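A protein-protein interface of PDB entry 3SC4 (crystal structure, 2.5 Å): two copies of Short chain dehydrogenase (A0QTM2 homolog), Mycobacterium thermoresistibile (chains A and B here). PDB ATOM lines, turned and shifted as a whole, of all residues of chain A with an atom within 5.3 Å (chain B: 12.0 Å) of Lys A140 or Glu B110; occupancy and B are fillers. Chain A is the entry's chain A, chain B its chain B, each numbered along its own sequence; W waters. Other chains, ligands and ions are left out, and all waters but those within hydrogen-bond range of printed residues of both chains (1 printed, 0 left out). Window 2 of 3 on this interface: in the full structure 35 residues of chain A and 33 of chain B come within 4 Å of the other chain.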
ATOM      1  N   GLN A 133     -14.563 -24.836 -24.844  1.00  0.00           N
ATOM      2  CA  GLN A 133     -14.569 -24.146 -23.566  1.00  0.00           C
ATOM      3  C   GLN A 133     -15.993 -24.065 -23.019  1.00  0.00           C
ATOM      4  O   GLN A 133     -16.245 -24.290 -21.824  1.00  0.00           O
ATOM      5  CB  GLN A 133     -14.007 -22.732 -23.706  1.00  0.00           C
ATOM      6  CG  GLN A 133     -14.153 -21.913 -22.453  1.00  0.00           C
ATOM      7  CD  GLN A 133     -13.613 -20.512 -22.617  1.00  0.00           C
ATOM      8  OE1 GLN A 133     -14.266 -19.658 -23.256  1.00  0.00           O
ATOM      9  NE2 GLN A 133     -12.431 -20.245 -22.023  1.00  0.00           N
ATOM     10  N   ILE A 136     -17.571 -27.679 -22.014  1.00  0.00           N
ATOM     11  CA  ILE A 136     -16.894 -28.379 -20.902  1.00  0.00           C
ATOM     12  C   ILE A 136     -17.582 -28.380 -19.512  1.00  0.00           C
ATOM     13  O   ILE A 136     -17.687 -29.416 -18.897  1.00  0.00           O
ATOM     14  CB  ILE A 136     -15.421 -27.887 -20.781  1.00  0.00           C
ATOM     15  CG1 ILE A 136     -14.572 -28.610 -21.850  1.00  0.00           C
ATOM     16  CG2 ILE A 136     -14.876 -28.081 -19.365  1.00  0.00           C
ATOM     17  CD1 ILE A 136     -13.169 -28.064 -22.069  1.00  0.00           C
ATOM     18  N   PRO A 137     -18.074 -27.240 -19.026  1.00  0.00           N
ATOM     19  CA  PRO A 137     -18.743 -27.298 -17.719  1.00  0.00           C
ATOM     20  C   PRO A 137     -19.947 -28.227 -17.670  1.00  0.00           C
ATOM     21  O   PRO A 137     -20.254 -28.788 -16.642  1.00  0.00           O
ATOM     22  CB  PRO A 137     -19.180 -25.844 -17.468  1.00  0.00           C
ATOM     23  CG  PRO A 137     -18.305 -25.002 -18.389  1.00  0.00           C
ATOM     24  CD  PRO A 137     -18.013 -25.873 -19.566  1.00  0.00           C
ATOM     25  N   HIS A 138     -20.602 -28.410 -18.802  1.00  0.00           N
ATOM     26  CA  HIS A 138     -21.829 -29.184 -18.873  1.00  0.00           C
ATOM     27  C   HIS A 138     -21.553 -30.633 -19.201  1.00  0.00           C
ATOM     28  O   HIS A 138     -22.482 -31.384 -19.452  1.00  0.00           O
ATOM     29  CB  HIS A 138     -22.728 -28.569 -19.940  1.00  0.00           C
ATOM     30  CG  HIS A 138     -23.020 -27.117 -19.719  1.00  0.00           C
ATOM     31  ND1 HIS A 138     -23.994 -26.678 -18.845  1.00  0.00           N
ATOM     32  CD2 HIS A 138     -22.462 -26.002 -20.245  1.00  0.00           C
ATOM     33  CE1 HIS A 138     -24.032 -25.356 -18.855  1.00  0.00           C
ATOM     34  NE2 HIS A 138     -23.109 -24.921 -19.691  1.00  0.00           N
ATOM     35  N   MET A 139     -20.281 -31.020 -19.232  1.00  0.00           N
ATOM     36  CA  MET A 139     -19.872 -32.390 -19.536  1.00  0.00           C
ATOM     37  C   MET A 139     -19.233 -33.061 -18.315  1.00  0.00           C
ATOM     38  O   MET A 139     -18.979 -34.261 -18.325  1.00  0.00           O
ATOM     39  CB  MET A 139     -18.842 -32.403 -20.685  1.00  0.00           C
ATOM     40  CG  MET A 139     -19.231 -31.637 -21.930  1.00  0.00           C
ATOM     41  SD  MET A 139     -17.924 -31.651 -23.194  1.00  0.00           S
ATOM     42  CE  MET A 139     -17.957 -33.375 -23.696  1.00  0.00           C
ATOM     43  N   LYS A 140     -18.932 -32.274 -17.294  1.00  0.00           N
ATOM     44  CA  LYS A 140     -18.353 -32.777 -16.051  1.00  0.00           C
ATOM     45  C   LYS A 140     -19.103 -33.842 -15.251  1.00  0.00           C
ATOM     46  O   LYS A 140     -18.468 -34.655 -14.581  1.00  0.00           O
ATOM     47  CB  LYS A 140     -17.997 -31.595 -15.150  1.00  0.00           C
ATOM     48  CG  LYS A 140     -16.703 -30.936 -15.581  1.00  0.00           C
ATOM     49  CD  LYS A 140     -16.408 -29.699 -14.783  1.00  0.00           C
ATOM     50  CE  LYS A 140     -15.076 -29.090 -15.147  1.00  0.00           C
ATOM     51  NZ  LYS A 140     -14.593 -28.176 -14.094  1.00  0.00           N
ATOM     52  N   GLY A 141     -20.420 -33.887 -15.319  1.00  0.00           N
ATOM     53  CA  GLY A 141     -21.127 -34.883 -14.511  1.00  0.00           C
ATOM     54  C   GLY A 141     -21.234 -36.278 -15.123  1.00  0.00           C
ATOM     55  O   GLY A 141     -21.558 -37.238 -14.430  1.00  0.00           O
ATOM     56  N   ARG A 142     -20.915 -36.395 -16.408  1.00  0.00           N
ATOM     57  CA  ARG A 142     -21.606 -37.345 -17.262  1.00  0.00           C
ATOM     58  C   ARG A 142     -20.893 -38.701 -17.276  1.00  0.00           C
ATOM     59  O   ARG A 142     -19.777 -38.848 -16.731  1.00  0.00           O
ATOM     60  CB  ARG A 142     -21.762 -36.757 -18.663  1.00  0.00           C
ATOM     61  CG  ARG A 142     -22.142 -35.242 -18.668  1.00  0.00           C
ATOM     62  CD  ARG A 142     -23.587 -34.992 -18.334  1.00  0.00           C
ATOM     63  NE  ARG A 142     -24.432 -35.622 -19.334  1.00  0.00           N
ATOM     64  CZ  ARG A 142     -25.768 -35.602 -19.334  1.00  0.00           C
ATOM     65  NH1 ARG A 142     -26.442 -36.243 -20.300  1.00  0.00           N
ATOM     66  NH2 ARG A 142     -26.436 -34.947 -18.384  1.00  0.00           N
ATOM     67  N   GLU A 183      -5.592 -30.924 -19.765  1.00  0.00           N
ATOM     68  CA  GLU A 183      -6.156 -30.056 -18.754  1.00  0.00           C
ATOM     69  C   GLU A 183      -7.435 -30.656 -18.169  1.00  0.00           C
ATOM     70  O   GLU A 183      -7.764 -30.445 -16.992  1.00  0.00           O
ATOM     71  CB  GLU A 183      -6.366 -28.674 -19.323  1.00  0.00           C
ATOM     72  CG  GLU A 183      -5.049 -27.967 -19.588  1.00  0.00           C
ATOM     73  CD  GLU A 183      -5.214 -26.560 -20.181  1.00  0.00           C
ATOM     74  OE1 GLU A 183      -6.265 -26.230 -20.820  1.00  0.00           O
ATOM     75  OE2 GLU A 183      -4.245 -25.787 -20.021  1.00  0.00           O
ATOM     76  N   LEU A 184      -8.134 -31.455 -18.953  1.00  0.00           N
ATOM     77  CA  LEU A 184      -9.401 -31.943 -18.490  1.00  0.00           C
ATOM     78  C   LEU A 184      -9.316 -33.405 -18.046  1.00  0.00           C
ATOM     79  O   LEU A 184     -10.323 -34.006 -17.706  1.00  0.00           O
ATOM     80  CB  LEU A 184     -10.500 -31.661 -19.536  1.00  0.00           C
ATOM     81  CG  LEU A 184     -11.180 -30.260 -19.474  1.00  0.00           C
ATOM     82  CD1 LEU A 184     -11.930 -30.061 -18.173  1.00  0.00           C
ATOM     83  CD2 LEU A 184     -10.216 -29.144 -19.630  1.00  0.00           C
ATOM     84  N   ALA A 187     -10.906 -34.381 -14.783  1.00  0.00           N
ATOM     85  CA  ALA A 187     -12.347 -34.159 -14.784  1.00  0.00           C
ATOM     86  C   ALA A 187     -13.330 -35.276 -15.221  1.00  0.00           C
ATOM     87  O   ALA A 187     -14.539 -35.120 -14.999  1.00  0.00           O
ATOM     88  CB  ALA A 187     -12.686 -32.844 -15.470  1.00  0.00           C
ATOM     89  N   ILE A 189     -12.755 -35.568 -18.926  1.00  0.00           N
ATOM     90  CA  ILE A 189     -13.425 -35.442 -20.198  1.00  0.00           C
ATOM     91  C   ILE A 189     -12.372 -35.848 -21.214  1.00  0.00           C
ATOM     92  O   ILE A 189     -11.268 -35.306 -21.203  1.00  0.00           O
ATOM     93  CB  ILE A 189     -13.882 -33.965 -20.401  1.00  0.00           C
ATOM     94  CG1 ILE A 189     -14.892 -33.591 -19.311  1.00  0.00           C
ATOM     95  CG2 ILE A 189     -14.456 -33.757 -21.779  1.00  0.00           C
ATOM     96  CD1 ILE A 189     -15.066 -32.099 -19.097  1.00  0.00           C
ATOM     97  N   ASN B 105      -0.488 -15.689 -20.621  1.00  0.00           N
ATOM     98  CA  ASN B 105      -1.377 -16.031 -19.533  1.00  0.00           C
ATOM     99  C   ASN B 105      -1.218 -17.550 -19.414  1.00  0.00           C
ATOM    100  O   ASN B 105      -1.238 -18.238 -20.433  1.00  0.00           O
ATOM    101  CB  ASN B 105      -2.815 -15.639 -19.831  1.00  0.00           C
ATOM    102  CG  ASN B 105      -3.801 -16.090 -18.752  1.00  0.00           C
ATOM    103  OD1 ASN B 105      -3.668 -17.161 -18.173  1.00  0.00           O
ATOM    104  ND2 ASN B 105      -4.817 -15.288 -18.523  1.00  0.00           N
ATOM    105  N   LEU B 106      -1.030 -18.053 -18.192  1.00  0.00           N
ATOM    106  CA  LEU B 106      -0.625 -19.445 -18.009  1.00  0.00           C
ATOM    107  C   LEU B 106      -1.782 -20.271 -17.454  1.00  0.00           C
ATOM    108  O   LEU B 106      -1.581 -21.373 -16.921  1.00  0.00           O
ATOM    109  CB  LEU B 106       0.618 -19.545 -17.093  1.00  0.00           C
ATOM    110  CG  LEU B 106       1.857 -18.749 -17.564  1.00  0.00           C
ATOM    111  CD1 LEU B 106       3.047 -18.961 -16.624  1.00  0.00           C
ATOM    112  CD2 LEU B 106       2.266 -19.147 -18.967  1.00  0.00           C
ATOM    113  N   GLY B 107      -2.996 -19.744 -17.570  1.00  0.00           N
ATOM    114  CA  GLY B 107      -4.170 -20.471 -17.098  1.00  0.00           C
ATOM    115  C   GLY B 107      -4.619 -21.519 -18.094  1.00  0.00           C
ATOM    116  O   GLY B 107      -4.140 -21.557 -19.237  1.00  0.00           O
ATOM    117  N   SER B 108      -5.556 -22.353 -17.656  1.00  0.00           N
ATOM    118  CA  SER B 108      -6.144 -23.377 -18.486  1.00  0.00           C
ATOM    119  C   SER B 108      -7.291 -22.833 -19.333  1.00  0.00           C
ATOM    120  O   SER B 108      -7.690 -21.695 -19.186  1.00  0.00           O
ATOM    121  CB  SER B 108      -6.683 -24.494 -17.603  1.00  0.00           C
ATOM    122  OG  SER B 108      -7.965 -24.169 -17.067  1.00  0.00           O
ATOM    123  N   ILE B 109      -7.833 -23.675 -20.213  1.00  0.00           N
ATOM    124  CA  ILE B 109      -9.004 -23.336 -21.008  1.00  0.00           C
ATOM    125  C   ILE B 109     -10.195 -22.958 -20.119  1.00  0.00           C
ATOM    126  O   ILE B 109     -11.060 -22.152 -20.494  1.00  0.00           O
ATOM    127  CB  ILE B 109      -9.353 -24.499 -21.944  1.00  0.00           C
ATOM    128  CG1 ILE B 109     -10.587 -24.182 -22.805  1.00  0.00           C
ATOM    129  CG2 ILE B 109      -9.571 -25.794 -21.171  1.00  0.00           C
ATOM    130  CD1 ILE B 109     -10.657 -25.032 -24.125  1.00  0.00           C
ATOM    131  N   GLU B 110     -10.252 -23.555 -18.937  1.00  0.00           N
ATOM    132  CA  GLU B 110     -11.309 -23.250 -17.990  1.00  0.00           C
ATOM    133  C   GLU B 110     -11.158 -21.852 -17.390  1.00  0.00           C
ATOM    134  O   GLU B 110     -12.132 -21.290 -16.965  1.00  0.00           O
ATOM    135  CB  GLU B 110     -11.335 -24.285 -16.860  1.00  0.00           C
ATOM    136  CG  GLU B 110     -11.600 -25.689 -17.363  1.00  0.00           C
ATOM    137  CD  GLU B 110     -11.811 -26.705 -16.246  1.00  0.00           C
ATOM    138  OE1 GLU B 110     -10.816 -27.173 -15.667  1.00  0.00           O
ATOM    139  OE2 GLU B 110     -12.981 -27.048 -15.968  1.00  0.00           O
ATOM    140  N   GLU B 111      -9.944 -21.309 -17.366  1.00  0.00           N
ATOM    141  CA  GLU B 111      -9.627 -20.052 -16.677  1.00  0.00           C
ATOM    142  C   GLU B 111      -9.423 -18.850 -17.596  1.00  0.00           C
ATOM    143  O   GLU B 111      -9.532 -17.714 -17.122  1.00  0.00           O
ATOM    144  CB  GLU B 111      -8.326 -20.222 -15.863  1.00  0.00           C
ATOM    145  CG  GLU B 111      -8.462 -21.280 -14.754  1.00  0.00           C
ATOM    146  CD  GLU B 111      -7.135 -21.777 -14.152  1.00  0.00           C
ATOM    147  OE1 GLU B 111      -6.066 -21.800 -14.838  1.00  0.00           O
ATOM    148  OE2 GLU B 111      -7.193 -22.190 -12.957  1.00  0.00           O
ATOM    149  N   VAL B 112      -9.105 -19.088 -18.884  1.00  0.00           N
ATOM    150  CA  VAL B 112      -8.720 -18.028 -19.818  1.00  0.00           C
ATOM    151  C   VAL B 112      -9.904 -17.697 -20.738  1.00  0.00           C
ATOM    152  O   VAL B 112     -10.230 -18.460 -21.648  1.00  0.00           O
ATOM    153  CB  VAL B 112      -7.490 -18.424 -20.640  1.00  0.00           C
ATOM    154  CG1 VAL B 112      -7.221 -17.398 -21.746  1.00  0.00           C
ATOM    155  CG2 VAL B 112      -6.239 -18.570 -19.728  1.00  0.00           C
ATOM    156  N   PRO B 113     -10.578 -16.561 -20.494  1.00  0.00           N
ATOM    157  CA  PRO B 113     -11.733 -16.272 -21.370  1.00  0.00           C
ATOM    158  C   PRO B 113     -11.331 -15.979 -22.802  1.00  0.00           C
ATOM    159  O   PRO B 113     -10.164 -15.677 -23.097  1.00  0.00           O
ATOM    160  CB  PRO B 113     -12.381 -15.012 -20.755  1.00  0.00           C
ATOM    161  CG  PRO B 113     -11.667 -14.764 -19.439  1.00  0.00           C
ATOM    162  CD  PRO B 113     -10.379 -15.547 -19.434  1.00  0.00           C
ATOM    163  N   LEU B 114     -12.311 -16.042 -23.671  1.00  0.00           N
ATOM    164  CA  LEU B 114     -12.102 -15.860 -25.088  1.00  0.00           C
ATOM    165  C   LEU B 114     -11.365 -14.542 -25.400  1.00  0.00           C
ATOM    166  O   LEU B 114     -10.501 -14.496 -26.259  1.00  0.00           O
ATOM    167  CB  LEU B 114     -13.467 -15.937 -25.787  1.00  0.00           C
ATOM    168  CG  LEU B 114     -13.507 -16.356 -27.245  1.00  0.00           C
ATOM    169  CD1 LEU B 114     -12.682 -17.650 -27.562  1.00  0.00           C
ATOM    170  CD2 LEU B 114     -14.987 -16.474 -27.624  1.00  0.00           C
ATOM    171  N   LYS B 115     -11.680 -13.480 -24.670  1.00  0.00           N
ATOM    172  CA  LYS B 115     -11.069 -12.162 -24.903  1.00  0.00           C
ATOM    173  C   LYS B 115      -9.558 -12.203 -24.638  1.00  0.00           C
ATOM    174  O   LYS B 115      -8.766 -11.593 -25.343  1.00  0.00           O
ATOM    175  CB  LYS B 115     -11.763 -11.119 -24.020  1.00  0.00           C
ATOM    176  CG  LYS B 115     -11.222  -9.652 -24.120  1.00  0.00           C
ATOM    177  CD  LYS B 115     -11.956  -8.682 -23.107  1.00  0.00           C
ATOM    178  CE  LYS B 115     -12.851  -7.603 -23.787  1.00  0.00           C
ATOM    179  NZ  LYS B 115     -12.138  -6.269 -24.031  1.00  0.00           N
ATOM    180  N   ARG B 116      -9.160 -12.943 -23.619  1.00  0.00           N
ATOM    181  CA  ARG B 116      -7.746 -13.102 -23.334  1.00  0.00           C
ATOM    182  C   ARG B 116      -7.082 -13.992 -24.379  1.00  0.00           C
ATOM    183  O   ARG B 116      -5.981 -13.710 -24.825  1.00  0.00           O
ATOM    184  CB  ARG B 116      -7.564 -13.699 -21.956  1.00  0.00           C
ATOM    185  CG  ARG B 116      -6.132 -14.003 -21.589  1.00  0.00           C
ATOM    186  CD  ARG B 116      -5.246 -12.764 -21.545  1.00  0.00           C
ATOM    187  NE  ARG B 116      -5.728 -11.750 -20.601  1.00  0.00           N
ATOM    188  CZ  ARG B 116      -5.005 -10.710 -20.210  1.00  0.00           C
ATOM    189  NH1 ARG B 116      -5.517  -9.858 -19.344  1.00  0.00           N
ATOM    190  NH2 ARG B 116      -3.771 -10.519 -20.676  1.00  0.00           N
ATOM    191  N   PHE B 117      -7.768 -15.068 -24.752  1.00  0.00           N
ATOM    192  CA  PHE B 117      -7.298 -15.947 -25.815  1.00  0.00           C
ATOM    193  C   PHE B 117      -7.006 -15.152 -27.077  1.00  0.00           C
ATOM    194  O   PHE B 117      -5.956 -15.325 -27.668  1.00  0.00           O
ATOM    195  CB  PHE B 117      -8.340 -17.035 -26.116  1.00  0.00           C
ATOM    196  CG  PHE B 117      -7.978 -17.911 -27.264  1.00  0.00           C
ATOM    197  CD1 PHE B 117      -7.336 -19.112 -27.048  1.00  0.00           C
ATOM    198  CD2 PHE B 117      -8.273 -17.524 -28.569  1.00  0.00           C
ATOM    199  CE1 PHE B 117      -6.988 -19.926 -28.101  1.00  0.00           C
ATOM    200  CE2 PHE B 117      -7.932 -18.327 -29.631  1.00  0.00           C
ATOM    201  CZ  PHE B 117      -7.280 -19.533 -29.402  1.00  0.00           C
ATOM    202  N   MET B 120      -3.866 -13.214 -27.120  1.00  0.00           N
ATOM    203  CA  MET B 120      -2.695 -14.071 -27.344  1.00  0.00           C
ATOM    204  C   MET B 120      -2.570 -14.563 -28.809  1.00  0.00           C
ATOM    205  O   MET B 120      -1.502 -14.512 -29.406  1.00  0.00           O
ATOM    206  CB  MET B 120      -2.734 -15.287 -26.391  1.00  0.00           C
ATOM    207  CG  MET B 120      -2.567 -14.935 -24.921  1.00  0.00           C
ATOM    208  SD  MET B 120      -2.190 -16.318 -23.820  1.00  0.00           S
ATOM    209  CE  MET B 120      -3.843 -16.600 -23.314  1.00  0.00           C
ATOM    210  N   LEU B 161       2.030 -30.010 -23.432  1.00  0.00           N
ATOM    211  CA  LEU B 161       0.846 -29.548 -24.129  1.00  0.00           C
ATOM    212  C   LEU B 161      -0.064 -28.751 -23.195  1.00  0.00           C
ATOM    213  O   LEU B 161      -1.250 -28.900 -23.195  1.00  0.00           O
ATOM    214  CB  LEU B 161       0.107 -30.728 -24.777  1.00  0.00           C
ATOM    215  CG  LEU B 161       0.924 -31.401 -25.887  1.00  0.00           C
ATOM    216  CD1 LEU B 161       0.273 -32.697 -26.407  1.00  0.00           C
ATOM    217  CD2 LEU B 161       1.182 -30.449 -27.028  1.00  0.00           C
ATOM    218  N   ARG B 162       0.520 -27.817 -22.485  1.00  0.00           N
ATOM    219  CA  ARG B 162      -0.075 -27.218 -21.304  1.00  0.00           C
ATOM    220  C   ARG B 162       0.755 -25.960 -21.029  1.00  0.00           C
ATOM    221  O   ARG B 162       1.973 -25.976 -21.264  1.00  0.00           O
ATOM    222  CB  ARG B 162       0.139 -28.170 -20.149  1.00  0.00           C
ATOM    223  CG  ARG B 162      -1.027 -28.348 -19.234  1.00  0.00           C
ATOM    224  CD  ARG B 162      -0.785 -29.503 -18.227  1.00  0.00           C
ATOM    225  NE  ARG B 162      -1.855 -29.524 -17.235  1.00  0.00           N
ATOM    226  CZ  ARG B 162      -1.999 -30.430 -16.272  1.00  0.00           C
ATOM    227  NH1 ARG B 162      -1.146 -31.436 -16.148  1.00  0.00           N
ATOM    228  NH2 ARG B 162      -3.014 -30.324 -15.423  1.00  0.00           N
ATOM    229  N   PRO B 163       0.134 -24.853 -20.597  1.00  0.00           N
ATOM    230  CA  PRO B 163      -1.302 -24.629 -20.558  1.00  0.00           C
ATOM    231  C   PRO B 163      -1.750 -24.290 -21.949  1.00  0.00           C
ATOM    232  O   PRO B 163      -1.012 -23.712 -22.706  1.00  0.00           O
ATOM    233  CB  PRO B 163      -1.456 -23.453 -19.590  1.00  0.00           C
ATOM    234  CG  PRO B 163      -0.177 -22.741 -19.661  1.00  0.00           C
ATOM    235  CD  PRO B 163       0.899 -23.717 -20.063  1.00  0.00           C
ATOM    236  N   THR B 164      -2.981 -24.630 -22.256  1.00  0.00           N
ATOM    237  CA  THR B 164      -3.461 -24.727 -23.635  1.00  0.00           C
ATOM    238  C   THR B 164      -3.476 -23.416 -24.424  1.00  0.00           C
ATOM    239  O   THR B 164      -2.915 -23.333 -25.493  1.00  0.00           O
ATOM    240  CB  THR B 164      -4.830 -25.404 -23.641  1.00  0.00           C
ATOM    241  OG1 THR B 164      -4.665 -26.719 -23.096  1.00  0.00           O
ATOM    242  CG2 THR B 164      -5.388 -25.473 -25.033  1.00  0.00           C
ATOM    243  N   PRO B 165      -4.083 -22.376 -23.886  1.00  0.00           N
ATOM    244  CA  PRO B 165      -4.097 -21.122 -24.642  1.00  0.00           C
ATOM    245  C   PRO B 165      -2.718 -20.637 -25.044  1.00  0.00           C
ATOM    246  O   PRO B 165      -2.470 -20.313 -26.211  1.00  0.00           O
ATOM    247  CB  PRO B 165      -4.746 -20.133 -23.659  1.00  0.00           C
ATOM    248  CG  PRO B 165      -5.527 -21.013 -22.727  1.00  0.00           C
ATOM    249  CD  PRO B 165      -4.725 -22.244 -22.574  1.00  0.00           C
ATOM    250  N   TYR B 166      -1.821 -20.562 -24.085  1.00  0.00           N
ATOM    251  CA  TYR B 166      -0.472 -20.067 -24.336  1.00  0.00           C
ATOM    252  C   TYR B 166       0.318 -21.020 -25.220  1.00  0.00           C
ATOM    253  O   TYR B 166       1.003 -20.577 -26.115  1.00  0.00           O
ATOM    254  CB  TYR B 166       0.266 -19.817 -23.008  1.00  0.00           C
ATOM    255  CG  TYR B 166       1.591 -19.119 -23.135  1.00  0.00           C
ATOM    256  CD1 TYR B 166       1.685 -17.872 -23.714  1.00  0.00           C
ATOM    257  CD2 TYR B 166       2.738 -19.700 -22.643  1.00  0.00           C
ATOM    258  CE1 TYR B 166       2.933 -17.220 -23.830  1.00  0.00           C
ATOM    259  CE2 TYR B 166       3.969 -19.086 -22.744  1.00  0.00           C
ATOM    260  CZ  TYR B 166       4.082 -17.846 -23.352  1.00  0.00           C
ATOM    261  OH  TYR B 166       5.327 -17.232 -23.433  1.00  0.00           O
ATOM    262  N   MET B 168      -0.899 -23.002 -27.425  1.00  0.00           N
ATOM    263  CA  MET B 168      -1.450 -22.830 -28.784  1.00  0.00           C
ATOM    264  C   MET B 168      -0.833 -21.622 -29.504  1.00  0.00           C
ATOM    265  O   MET B 168      -0.519 -21.682 -30.703  1.00  0.00           O
ATOM    266  CB  MET B 168      -2.985 -22.663 -28.751  1.00  0.00           C
ATOM    267  CG  MET B 168      -3.702 -23.956 -28.557  1.00  0.00           C
ATOM    268  SD  MET B 168      -5.458 -23.708 -28.278  1.00  0.00           S
ATOM    269  CE  MET B 168      -5.955 -23.052 -29.885  1.00  0.00           C
HETATM  270  O   HOH W   1     -14.573 -17.037 -22.772  1.00  0.00           O
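N of Ile B109 sits at hydrogen-bond distance from OE1 of Glu A183, at 3.1 Å.
NE2 of Gln A133 lies within hydrogen-bond range of O of Val B112.
The side-chain amide nitrogen of Gln A133 is in hydrogen-bond range of the backbone carbonyl oxygen of Ile B109, at 2.8 Å.
The backbone NH (N) of Thr B164 is in hydrogen-bond range of the side-chain carboxylate (OE2) of Glu A183, at 2.8 Å.
OE2 of Glu B110 is in salt-bridge range of NZ of Lys A140 (2.7 Å).
The side-chain hydroxyl (OG) of Ser B108 is in hydrogen-bond range of the backbone NH (N) of Glu B110 (3.0 Å).
The backbone NH (N) of Ser B108 lies within hydrogen-bond range of the side-chain carboxylate (OE1) of Glu B111.
N of Ile A189 sits at hydrogen-bond distance from O of Leu A184 (3.1 Å).
Among the printed residues, merely in contact across the chains: Glu A183 with Ser B108 (3.4 Å), Glu A183 with Pro B163 (3.2 Å), Leu A184 with Ile B109 (3.7 Å) and Leu A184 with Glu B110 (3.9 Å).
Gln A133 touches just these residues of chain B: Ile B109 (2.8 Å) and Val B112 (2.9 Å).
No residue of chain B comes within 4 Å of Met A139.
Of the printed residues of chain B, Lys A140 touches Glu B110 (2.7 Å).
Printed residues of chain B within 4 Å of Glu A183: Ser B108 (3.4 Å), Ile B109 (3.1 Å), Pro B163 (3.2 Å) and Thr B164 (2.8 Å).
No residue of chain B comes within 4 Å of Ala A187.
Gly B107 touches none of the printed residues of chain A.
Of the printed residues of chain A, Glu B110 touches Lys A140 (2.7 Å) and Leu A184 (3.9 Å).
Of the printed residues of chain A, Val B112 touches Gln A133.
Arg B116 touches none of the printed residues of chain A.
Of the printed residues of chain A, Pro B163 touches Glu A183 (3.2 Å).
The nearest printed residue of chain B that does not touch Lys A140 is Ser B108 (8.3 Å).
Hydrophobic or aromatic side chains of chain A that line the printed part of chain B: Leu A184.
Of the 21 printed residues of chain B, 6 touch a printed residue of chain A.
Printed residues of chain B that touch a printed residue of chain A: Ser B108, Ile B109, Glu B110, Val B112, Pro B163 and Thr B164.
Hydrophobic or aromatic side chains of chain B within 4 Å of the printed part of chain A: Ile B109 and Pro B163.
No position is printed for both chains.
Of the 9 pairs that touch across the chains among the printed residues, none has its exchanged pair printed and touching as well.
Water W1 lies within hydrogen-bond range of the backbone NH (N) of Leu B114 (2.6 Å) and the side-chain amide oxygen (OE1) of Gln A133 (2.7 Å).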
